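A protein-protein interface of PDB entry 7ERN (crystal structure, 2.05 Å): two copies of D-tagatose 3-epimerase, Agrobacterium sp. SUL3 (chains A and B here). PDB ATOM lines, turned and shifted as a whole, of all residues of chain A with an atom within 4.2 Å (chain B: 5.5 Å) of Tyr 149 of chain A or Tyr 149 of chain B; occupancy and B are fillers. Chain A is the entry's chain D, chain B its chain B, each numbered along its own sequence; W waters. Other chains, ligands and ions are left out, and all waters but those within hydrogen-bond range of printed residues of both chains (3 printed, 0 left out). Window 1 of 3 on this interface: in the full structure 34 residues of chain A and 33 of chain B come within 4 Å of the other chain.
The side-chain amide nitrogen (ND2) of Asn 147 of chain B lies within hydrogen-bond range of the side-chain hydroxyl (OH) of Tyr 149 of chain A (3.3 Å). O of Arg 148 of chain B lies within hydrogen-bond range of OG of Ser 252 of chain A (3.3 Å). The side-chain amide nitrogen (ND2) of Asn 147 of chain A lies within hydrogen-bond range of the side-chain hydroxyl (OH) of Tyr 149 of chain B, at 3.3 Å. OH of Tyr 149 of chain A lies within hydrogen-bond range of OE2 of Glu 150 of chain B, 2.6 Å away. The indole nitrogen (NE1) of Trp 254 of chain B lies within hydrogen-bond range of the backbone carbonyl oxygen (O) of Arg 148 of chain A (2.8 Å). The side-chain carboxylate (OE2) of Glu 150 of chain A sits close to the side-chain hydroxyl (OH) of Tyr 149 of chain B (2.3 Å).
N of Ser 108 of chain B lies within hydrogen-bond range of O of Glu 150 of chain B (3.2 Å). The backbone NH of Tyr 149 of chain B is in hydrogen-bond range of the side-chain amide oxygen of Asn 147 of chain B. The side-chain amide oxygen (OD1) of Asn 147 of chain B sits at hydrogen-bond distance from the backbone NH (N) of Glu 150 of chain B (3.4 Å). A ring nitrogen (ND1) of His 180 of chain B sits at hydrogen-bond distance from the side-chain amide nitrogen of Asn 147 of chain B. The guanidinium group of Arg 148 of chain B is in salt-bridge range of the side-chain carboxylate of Glu 184 of chain B. The side-chain amide oxygen (OD1) of Asn 147 of chain A is in hydrogen-bond range of the backbone NH (N) of Tyr 149 of chain A.
Among the printed residues, merely in contact across the chains: Arg 148 of chain A with Ser 252 of chain B (3.4 Å), Tyr 149 of chain A with Tyr 149 of chain B (3.4 Å), Tyr 149 of chain A with Phe 179 of chain B (3.6 Å), Tyr 149 of chain A with Ser 252 of chain B (3.8 Å), Asn 151 of chain A with Trp 254 of chain B (3.8 Å), Phe 179 of chain A with Tyr 149 of chain B (3.6 Å), Phe 179 of chain A with Met 183 of chain B (3.7 Å), Met 183 of chain A with Phe 179 of chain B (3.6 Å), Met 183 of chain A with Met 183 of chain B (3.5 Å) and Ser 252 of chain A with Tyr 149 of chain B (3.96 Å).
Printed residues of chain B within 4 Å of Tyr 149 of chain A: Asn 147 (3.3 Å), Tyr 149 (3.4 Å), Glu 150 (2.6 Å), Phe 179 (3.6 Å) and Ser 252 (3.8 Å). Ser 108 of chain B touches none of the printed residues of chain A. Of chain A, only Asn 147 (3.3 Å), Tyr 149 (3.4 Å), Glu 150 (2.3 Å), Phe 179 (3.6 Å) and Ser 252 (3.96 Å) come within 4 Å of Tyr 149 of chain B. Printed residues of chain A within 4 Å of Glu 150 of chain B: Tyr 149 (2.6 Å). Printed residues of chain A within 4 Å of Phe 179 of chain B: Tyr 149 (3.6 Å) and Met 183 (3.6 Å). Printed residues of chain A within 4 Å of Ser 252 of chain B: Arg 148 and Tyr 149. Printed residues of chain A within 4 Å of Trp 254 of chain B: Arg 148 and Asn 151.
Of the 8 printed residues of chain A, 8 touch a printed residue of chain B. Printed residues of chain A that touch a printed residue of chain B: Asn 147, Arg 148, Tyr 149, Glu 150, Asn 151, Phe 179, Met 183 and Ser 252. Hydrophobic or aromatic side chains of chain A that line the printed part of chain B: Tyr 149, Phe 179 and Met 183. Hydrophobic or aromatic side chains of chain B within 4 Å of the printed part of chain A: Tyr 149, Phe 179, Met 183 and Trp 254. Along chain B the printed residues that touch a printed residue of chain A span positions 147 to 254. Among the printed residues, no Asp or Glu carboxylate lies within 4 Å of a Lys or Arg side-chain nitrogen of the other chain.
Arg 148 of chain A touches Ser 252 of chain B, and with the chains exchanged Ser 252 of chain A touches Arg 148 of chain B. Tyr 149 of chain A touches Glu 150 of chain B, and with the chains exchanged Glu 150 of chain A touches Tyr 149 of chain B. Tyr 149 of chain A touches Phe 179 of chain B, and with the chains exchanged Phe 179 of chain A touches Tyr 149 of chain B. Phe 179 of chain A touches Met 183 of chain B, and with the chains exchanged Met 183 of chain A touches Phe 179 of chain B. Positions printed for both chains: 147, 148, 149, 150, 151, 179, 183 and 252.
Water W3 bridges OH of Tyr 149 of chain A (2.7 Å) and O of Ile 251 of chain B (2.9 Å). Water W2 lies within hydrogen-bond range of the side-chain carboxylate (OE2) of Glu 150 of chain B (2.8 Å) and the side-chain hydroxyl (OH) of Tyr 149 of chain A (3.4 Å). Water W1 lies within hydrogen-bond range of N of Trp 254 of chain B (2.9 Å) and NE of Arg 148 of chain A (3.4 Å).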
ATOM      1  N   ASN A 147      -3.326 -18.114  18.391  1.00  0.00           N
ATOM      2  CA  ASN A 147      -2.009 -18.506  17.900  1.00  0.00           C
ATOM      3  C   ASN A 147      -1.914 -18.364  16.375  1.00  0.00           C
ATOM      4  O   ASN A 147      -2.912 -18.209  15.669  1.00  0.00           O
ATOM      5  CB  ASN A 147      -1.659 -19.931  18.350  1.00  0.00           C
ATOM      6  CG  ASN A 147      -2.504 -21.001  17.676  1.00  0.00           C
ATOM      7  OD1 ASN A 147      -2.462 -21.165  16.464  1.00  0.00           O
ATOM      8  ND2 ASN A 147      -3.245 -21.767  18.474  1.00  0.00           N
ATOM      9  N   ARG A 148      -0.672 -18.426  15.880  1.00  0.00           N
ATOM     10  CA  ARG A 148      -0.343 -18.182  14.478  1.00  0.00           C
ATOM     11  C   ARG A 148      -1.090 -19.086  13.501  1.00  0.00           C
ATOM     12  O   ARG A 148      -1.219 -18.732  12.320  1.00  0.00           O
ATOM     13  CB  ARG A 148       1.164 -18.352  14.291  1.00  0.00           C
ATOM     14  CG  ARG A 148       1.659 -19.754  14.668  1.00  0.00           C
ATOM     15  CD  ARG A 148       3.148 -19.768  14.986  1.00  0.00           C
ATOM     16  NE  ARG A 148       3.472 -18.869  16.094  1.00  0.00           N
ATOM     17  CZ  ARG A 148       4.710 -18.610  16.491  1.00  0.00           C
ATOM     18  NH1 ARG A 148       5.733 -19.196  15.874  1.00  0.00           N
ATOM     19  NH2 ARG A 148       4.920 -17.772  17.501  1.00  0.00           N
ATOM     20  N   TYR A 149      -1.596 -20.236  13.947  1.00  0.00           N
ATOM     21  CA  TYR A 149      -2.284 -21.142  13.034  1.00  0.00           C
ATOM     22  C   TYR A 149      -3.753 -20.804  12.870  1.00  0.00           C
ATOM     23  O   TYR A 149      -4.381 -21.292  11.927  1.00  0.00           O
ATOM     24  CB  TYR A 149      -2.186 -22.599  13.515  1.00  0.00           C
ATOM     25  CG  TYR A 149      -0.785 -23.198  13.516  1.00  0.00           C
ATOM     26  CD1 TYR A 149      -0.232 -23.715  12.341  1.00  0.00           C
ATOM     27  CD2 TYR A 149      -0.023 -23.254  14.685  1.00  0.00           C
ATOM     28  CE1 TYR A 149       1.021 -24.258  12.321  1.00  0.00           C
ATOM     29  CE2 TYR A 149       1.255 -23.819  14.680  1.00  0.00           C
ATOM     30  CZ  TYR A 149       1.762 -24.324  13.493  1.00  0.00           C
ATOM     31  OH  TYR A 149       3.012 -24.886  13.429  1.00  0.00           O
ATOM     32  N   GLU A 150      -4.327 -20.010  13.775  1.00  0.00           N
ATOM     33  CA  GLU A 150      -5.735 -19.651  13.676  1.00  0.00           C
ATOM     34  C   GLU A 150      -5.947 -18.300  13.021  1.00  0.00           C
ATOM     35  O   GLU A 150      -6.999 -18.058  12.420  1.00  0.00           O
ATOM     36  CB  GLU A 150      -6.383 -19.643  15.074  1.00  0.00           C
ATOM     37  CG  GLU A 150      -6.193 -20.979  15.829  1.00  0.00           C
ATOM     38  CD  GLU A 150      -7.159 -21.161  16.997  1.00  0.00           C
ATOM     39  OE1 GLU A 150      -7.858 -20.179  17.377  1.00  0.00           O
ATOM     40  OE2 GLU A 150      -7.226 -22.294  17.535  1.00  0.00           O
ATOM     41  N   ASN A 151      -4.961 -17.423  13.126  1.00  0.00           N
ATOM     42  CA  ASN A 151      -5.113 -16.049  12.703  1.00  0.00           C
ATOM     43  C   ASN A 151      -3.718 -15.474  12.540  1.00  0.00           C
ATOM     44  O   ASN A 151      -2.776 -15.911  13.208  1.00  0.00           O
ATOM     45  CB  ASN A 151      -5.930 -15.270  13.733  1.00  0.00           C
ATOM     46  CG  ASN A 151      -6.217 -13.901  13.297  1.00  0.00           C
ATOM     47  OD1 ASN A 151      -5.413 -13.004  13.515  1.00  0.00           O
ATOM     48  ND2 ASN A 151      -7.365 -13.711  12.644  1.00  0.00           N
ATOM     49  N   PHE A 179      -3.573 -21.189  26.447  1.00  0.00           N
ATOM     50  CA  PHE A 179      -3.309 -22.152  25.384  1.00  0.00           C
ATOM     51  C   PHE A 179      -2.577 -21.485  24.229  1.00  0.00           C
ATOM     52  O   PHE A 179      -1.623 -22.044  23.680  1.00  0.00           O
ATOM     53  CB  PHE A 179      -4.611 -22.797  24.900  1.00  0.00           C
ATOM     54  CG  PHE A 179      -4.462 -23.626  23.629  1.00  0.00           C
ATOM     55  CD1 PHE A 179      -4.074 -24.954  23.691  1.00  0.00           C
ATOM     56  CD2 PHE A 179      -4.746 -23.076  22.375  1.00  0.00           C
ATOM     57  CE1 PHE A 179      -3.949 -25.728  22.530  1.00  0.00           C
ATOM     58  CE2 PHE A 179      -4.621 -23.829  21.209  1.00  0.00           C
ATOM     59  CZ  PHE A 179      -4.222 -25.166  21.289  1.00  0.00           C
ATOM     60  N   MET A 183       2.288 -20.932  23.048  1.00  0.00           N
ATOM     61  CA  MET A 183       3.016 -20.881  21.781  1.00  0.00           C
ATOM     62  C   MET A 183       3.527 -19.475  21.461  1.00  0.00           C
ATOM     63  O   MET A 183       4.691 -19.305  21.074  1.00  0.00           O
ATOM     64  CB  MET A 183       2.122 -21.379  20.635  1.00  0.00           C
ATOM     65  CG  MET A 183       2.790 -21.277  19.252  1.00  0.00           C
ATOM     66  SD  MET A 183       1.782 -21.955  17.899  1.00  0.00           S
ATOM     67  CE  MET A 183       1.756 -23.702  18.330  1.00  0.00           C
ATOM     68  N   SER A 252     -10.084 -27.735  15.024  1.00  0.00           N
ATOM     69  CA  SER A 252      -8.862 -28.461  14.665  1.00  0.00           C
ATOM     70  C   SER A 252      -8.434 -29.409  15.787  1.00  0.00           C
ATOM     71  O   SER A 252      -7.266 -29.471  16.174  1.00  0.00           O
ATOM     72  CB  SER A 252      -7.739 -27.482  14.297  1.00  0.00           C
ATOM     73  OG  SER A 252      -6.871 -28.064  13.339  1.00  0.00           O
ATOM     74  N   THR B 107       2.193 -30.513   6.189  1.00  0.00           N
ATOM     75  CA  THR B 107       2.121 -29.603   7.327  1.00  0.00           C
ATOM     76  C   THR B 107       1.026 -28.552   7.157  1.00  0.00           C
ATOM     77  O   THR B 107       0.940 -27.610   7.955  1.00  0.00           O
ATOM     78  CB  THR B 107       3.470 -28.920   7.546  1.00  0.00           C
ATOM     79  OG1 THR B 107       3.865 -28.251   6.346  1.00  0.00           O
ATOM     80  CG2 THR B 107       4.529 -29.950   7.938  1.00  0.00           C
ATOM     81  N   SER B 108       0.203 -28.688   6.124  1.00  0.00           N
ATOM     82  CA  SER B 108      -1.056 -27.969   5.996  1.00  0.00           C
ATOM     83  C   SER B 108      -2.169 -28.953   5.670  1.00  0.00           C
ATOM     84  O   SER B 108      -3.141 -28.605   4.995  1.00  0.00           O
ATOM     85  CB  SER B 108      -0.965 -26.897   4.914  1.00  0.00           C
ATOM     86  OG  SER B 108      -0.350 -27.461   3.772  1.00  0.00           O
ATOM     87  N   GLU B 109      -2.018 -30.191   6.122  1.00  0.00           N
ATOM     88  CA  GLU B 109      -2.917 -31.265   5.741  1.00  0.00           C
ATOM     89  C   GLU B 109      -4.050 -31.362   6.745  1.00  0.00           C
ATOM     90  O   GLU B 109      -3.822 -31.450   7.957  1.00  0.00           O
ATOM     91  CB  GLU B 109      -2.181 -32.605   5.657  1.00  0.00           C
ATOM     92  CG  GLU B 109      -3.127 -33.775   5.410  1.00  0.00           C
ATOM     93  CD  GLU B 109      -2.422 -35.046   4.978  1.00  0.00           C
ATOM     94  OE1 GLU B 109      -3.096 -35.916   4.385  1.00  0.00           O
ATOM     95  OE2 GLU B 109      -1.206 -35.190   5.250  1.00  0.00           O
ATOM     96  N   ASN B 147       1.879 -30.888  15.274  1.00  0.00           N
ATOM     97  CA  ASN B 147       0.706 -30.479  16.028  1.00  0.00           C
ATOM     98  C   ASN B 147      -0.567 -30.549  15.170  1.00  0.00           C
ATOM     99  O   ASN B 147      -0.536 -30.696  13.938  1.00  0.00           O
ATOM    100  CB  ASN B 147       0.914 -29.087  16.646  1.00  0.00           C
ATOM    101  CG  ASN B 147       0.827 -27.962  15.631  1.00  0.00           C
ATOM    102  OD1 ASN B 147      -0.191 -27.800  14.968  1.00  0.00           O
ATOM    103  ND2 ASN B 147       1.887 -27.158  15.532  1.00  0.00           N
ATOM    104  N   ARG B 148      -1.704 -30.452  15.870  1.00  0.00           N
ATOM    105  CA  ARG B 148      -3.024 -30.650  15.277  1.00  0.00           C
ATOM    106  C   ARG B 148      -3.330 -29.671  14.150  1.00  0.00           C
ATOM    107  O   ARG B 148      -4.207 -29.950  13.322  1.00  0.00           O
ATOM    108  CB  ARG B 148      -4.086 -30.500  16.362  1.00  0.00           C
ATOM    109  CG  ARG B 148      -4.042 -29.124  17.040  1.00  0.00           C
ATOM    110  CD  ARG B 148      -4.624 -29.167  18.435  1.00  0.00           C
ATOM    111  NE  ARG B 148      -3.984 -30.202  19.234  1.00  0.00           N
ATOM    112  CZ  ARG B 148      -4.406 -30.584  20.434  1.00  0.00           C
ATOM    113  NH1 ARG B 148      -5.477 -30.009  20.976  1.00  0.00           N
ATOM    114  NH2 ARG B 148      -3.755 -31.539  21.084  1.00  0.00           N
ATOM    115  N   TYR B 149      -2.659 -28.518  14.114  1.00  0.00           N
ATOM    116  CA  TYR B 149      -2.905 -27.549  13.060  1.00  0.00           C
ATOM    117  C   TYR B 149      -2.135 -27.856  11.785  1.00  0.00           C
ATOM    118  O   TYR B 149      -2.495 -27.333  10.728  1.00  0.00           O
ATOM    119  CB  TYR B 149      -2.531 -26.146  13.521  1.00  0.00           C
ATOM    120  CG  TYR B 149      -3.356 -25.584  14.657  1.00  0.00           C
ATOM    121  CD1 TYR B 149      -4.596 -25.012  14.419  1.00  0.00           C
ATOM    122  CD2 TYR B 149      -2.871 -25.584  15.967  1.00  0.00           C
ATOM    123  CE1 TYR B 149      -5.347 -24.466  15.455  1.00  0.00           C
ATOM    124  CE2 TYR B 149      -3.607 -25.041  17.005  1.00  0.00           C
ATOM    125  CZ  TYR B 149      -4.844 -24.475  16.741  1.00  0.00           C
ATOM    126  OH  TYR B 149      -5.587 -23.932  17.768  1.00  0.00           O
ATOM    127  N   GLU B 150      -1.076 -28.665  11.851  1.00  0.00           N
ATOM    128  CA  GLU B 150      -0.324 -28.970  10.639  1.00  0.00           C
ATOM    129  C   GLU B 150      -0.808 -30.234   9.945  1.00  0.00           C
ATOM    130  O   GLU B 150      -0.702 -30.352   8.711  1.00  0.00           O
ATOM    131  CB  GLU B 150       1.161 -29.104  10.969  1.00  0.00           C
ATOM    132  CG  GLU B 150       1.741 -27.846  11.609  1.00  0.00           C
ATOM    133  CD  GLU B 150       3.258 -27.804  11.552  1.00  0.00           C
ATOM    134  OE1 GLU B 150       3.874 -28.849  11.197  1.00  0.00           O
ATOM    135  OE2 GLU B 150       3.831 -26.730  11.863  1.00  0.00           O
ATOM    136  N   ASN B 151      -1.372 -31.158  10.707  1.00  0.00           N
ATOM    137  CA  ASN B 151      -1.675 -32.479  10.192  1.00  0.00           C
ATOM    138  C   ASN B 151      -2.630 -33.149  11.170  1.00  0.00           C
ATOM    139  O   ASN B 151      -2.517 -32.951  12.380  1.00  0.00           O
ATOM    140  CB  ASN B 151      -0.374 -33.273  10.044  1.00  0.00           C
ATOM    141  CG  ASN B 151      -0.590 -34.621   9.450  1.00  0.00           C
ATOM    142  OD1 ASN B 151      -0.856 -35.590  10.164  1.00  0.00           O
ATOM    143  ND2 ASN B 151      -0.478 -34.705   8.130  1.00  0.00           N
ATOM    144  N   PHE B 179       8.540 -28.354  20.004  1.00  0.00           N
ATOM    145  CA  PHE B 179       7.573 -27.319  19.652  1.00  0.00           C
ATOM    146  C   PHE B 179       6.181 -27.918  19.500  1.00  0.00           C
ATOM    147  O   PHE B 179       5.206 -27.368  20.010  1.00  0.00           O
ATOM    148  CB  PHE B 179       8.006 -26.610  18.372  1.00  0.00           C
ATOM    149  CG  PHE B 179       6.954 -25.693  17.798  1.00  0.00           C
ATOM    150  CD1 PHE B 179       6.801 -24.410  18.281  1.00  0.00           C
ATOM    151  CD2 PHE B 179       6.133 -26.118  16.761  1.00  0.00           C
ATOM    152  CE1 PHE B 179       5.818 -23.542  17.731  1.00  0.00           C
ATOM    153  CE2 PHE B 179       5.176 -25.275  16.224  1.00  0.00           C
ATOM    154  CZ  PHE B 179       5.017 -23.991  16.718  1.00  0.00           C
ATOM    155  N   HIS B 180       6.077 -29.062  18.823  1.00  0.00           N
ATOM    156  CA  HIS B 180       4.787 -29.718  18.645  1.00  0.00           C
ATOM    157  C   HIS B 180       4.323 -30.421  19.909  1.00  0.00           C
ATOM    158  O   HIS B 180       3.120 -30.415  20.217  1.00  0.00           O
ATOM    159  CB  HIS B 180       4.868 -30.712  17.490  1.00  0.00           C
ATOM    160  CG  HIS B 180       5.192 -30.064  16.183  1.00  0.00           C
ATOM    161  ND1 HIS B 180       4.439 -29.032  15.667  1.00  0.00           N
ATOM    162  CD2 HIS B 180       6.198 -30.275  15.305  1.00  0.00           C
ATOM    163  CE1 HIS B 180       4.957 -28.649  14.514  1.00  0.00           C
ATOM    164  NE2 HIS B 180       6.028 -29.385  14.273  1.00  0.00           N
ATOM    165  N   MET B 183       2.302 -28.580  22.643  1.00  0.00           N
ATOM    166  CA  MET B 183       0.850 -28.587  22.483  1.00  0.00           C
ATOM    167  C   MET B 183       0.253 -29.987  22.631  1.00  0.00           C
ATOM    168  O   MET B 183      -0.751 -30.168  23.323  1.00  0.00           O
ATOM    169  CB  MET B 183       0.472 -28.020  21.115  1.00  0.00           C
ATOM    170  CG  MET B 183      -1.007 -28.138  20.791  1.00  0.00           C
ATOM    171  SD  MET B 183      -1.454 -27.238  19.263  1.00  0.00           S
ATOM    172  CE  MET B 183      -0.899 -25.603  19.718  1.00  0.00           C
ATOM    173  N   GLU B 184       0.861 -30.983  21.988  1.00  0.00           N
ATOM    174  CA  GLU B 184       0.201 -32.269  21.812  1.00  0.00           C
ATOM    175  C   GLU B 184       0.306 -33.204  23.013  1.00  0.00           C
ATOM    176  O   GLU B 184      -0.538 -34.098  23.143  1.00  0.00           O
ATOM    177  CB  GLU B 184       0.754 -32.963  20.570  1.00  0.00           C
ATOM    178  CG  GLU B 184       0.407 -32.182  19.277  1.00  0.00           C
ATOM    179  CD  GLU B 184      -1.097 -31.935  19.120  1.00  0.00           C
ATOM    180  OE1 GLU B 184      -1.902 -32.838  19.455  1.00  0.00           O
ATOM    181  OE2 GLU B 184      -1.491 -30.841  18.651  1.00  0.00           O
ATOM    182  N   ILE B 251       5.272 -21.832   6.675  1.00  0.00           N
ATOM    183  CA  ILE B 251       5.545 -22.248   8.048  1.00  0.00           C
ATOM    184  C   ILE B 251       4.642 -21.548   9.054  1.00  0.00           C
ATOM    185  O   ILE B 251       4.899 -21.616  10.262  1.00  0.00           O
ATOM    186  CB  ILE B 251       7.027 -22.024   8.409  1.00  0.00           C
ATOM    187  CG1 ILE B 251       7.405 -20.550   8.209  1.00  0.00           C
ATOM    188  CG2 ILE B 251       7.903 -22.901   7.542  1.00  0.00           C
ATOM    189  CD1 ILE B 251       8.815 -20.206   8.663  1.00  0.00           C
ATOM    190  N   SER B 252       3.583 -20.884   8.576  1.00  0.00           N
ATOM    191  CA  SER B 252       2.642 -20.113   9.398  1.00  0.00           C
ATOM    192  C   SER B 252       3.365 -19.252  10.430  1.00  0.00           C
ATOM    193  O   SER B 252       3.008 -19.213  11.606  1.00  0.00           O
ATOM    194  CB  SER B 252       1.622 -21.028  10.089  1.00  0.00           C
ATOM    195  OG  SER B 252       0.953 -21.876   9.175  1.00  0.00           O
ATOM    196  N   TRP B 254       4.414 -15.431  11.178  1.00  0.00           N
ATOM    197  CA  TRP B 254       4.027 -14.107  10.705  1.00  0.00           C
ATOM    198  C   TRP B 254       4.861 -12.980  11.297  1.00  0.00           C
ATOM    199  O   TRP B 254       4.711 -11.837  10.860  1.00  0.00           O
ATOM    200  CB  TRP B 254       2.541 -13.855  11.001  1.00  0.00           C
ATOM    201  CG  TRP B 254       1.667 -15.034  10.709  1.00  0.00           C
ATOM    202  CD1 TRP B 254       0.867 -15.696  11.589  1.00  0.00           C
ATOM    203  CD2 TRP B 254       1.511 -15.698   9.441  1.00  0.00           C
ATOM    204  NE1 TRP B 254       0.214 -16.737  10.951  1.00  0.00           N
ATOM    205  CE2 TRP B 254       0.600 -16.762   9.634  1.00  0.00           C
ATOM    206  CE3 TRP B 254       2.059 -15.499   8.164  1.00  0.00           C
ATOM    207  CZ2 TRP B 254       0.215 -17.615   8.600  1.00  0.00           C
ATOM    208  CZ3 TRP B 254       1.678 -16.357   7.132  1.00  0.00           C
ATOM    209  CH2 TRP B 254       0.767 -17.401   7.359  1.00  0.00           C
HETATM  210  O   HOH W   1       4.108 -16.254  13.962  1.00  0.00           O
HETATM  211  O   HOH W   2       6.185 -25.352  12.332  1.00  0.00           O
HETATM  212  O   HOH W   3       5.086 -23.225  12.724  1.00  0.00           O
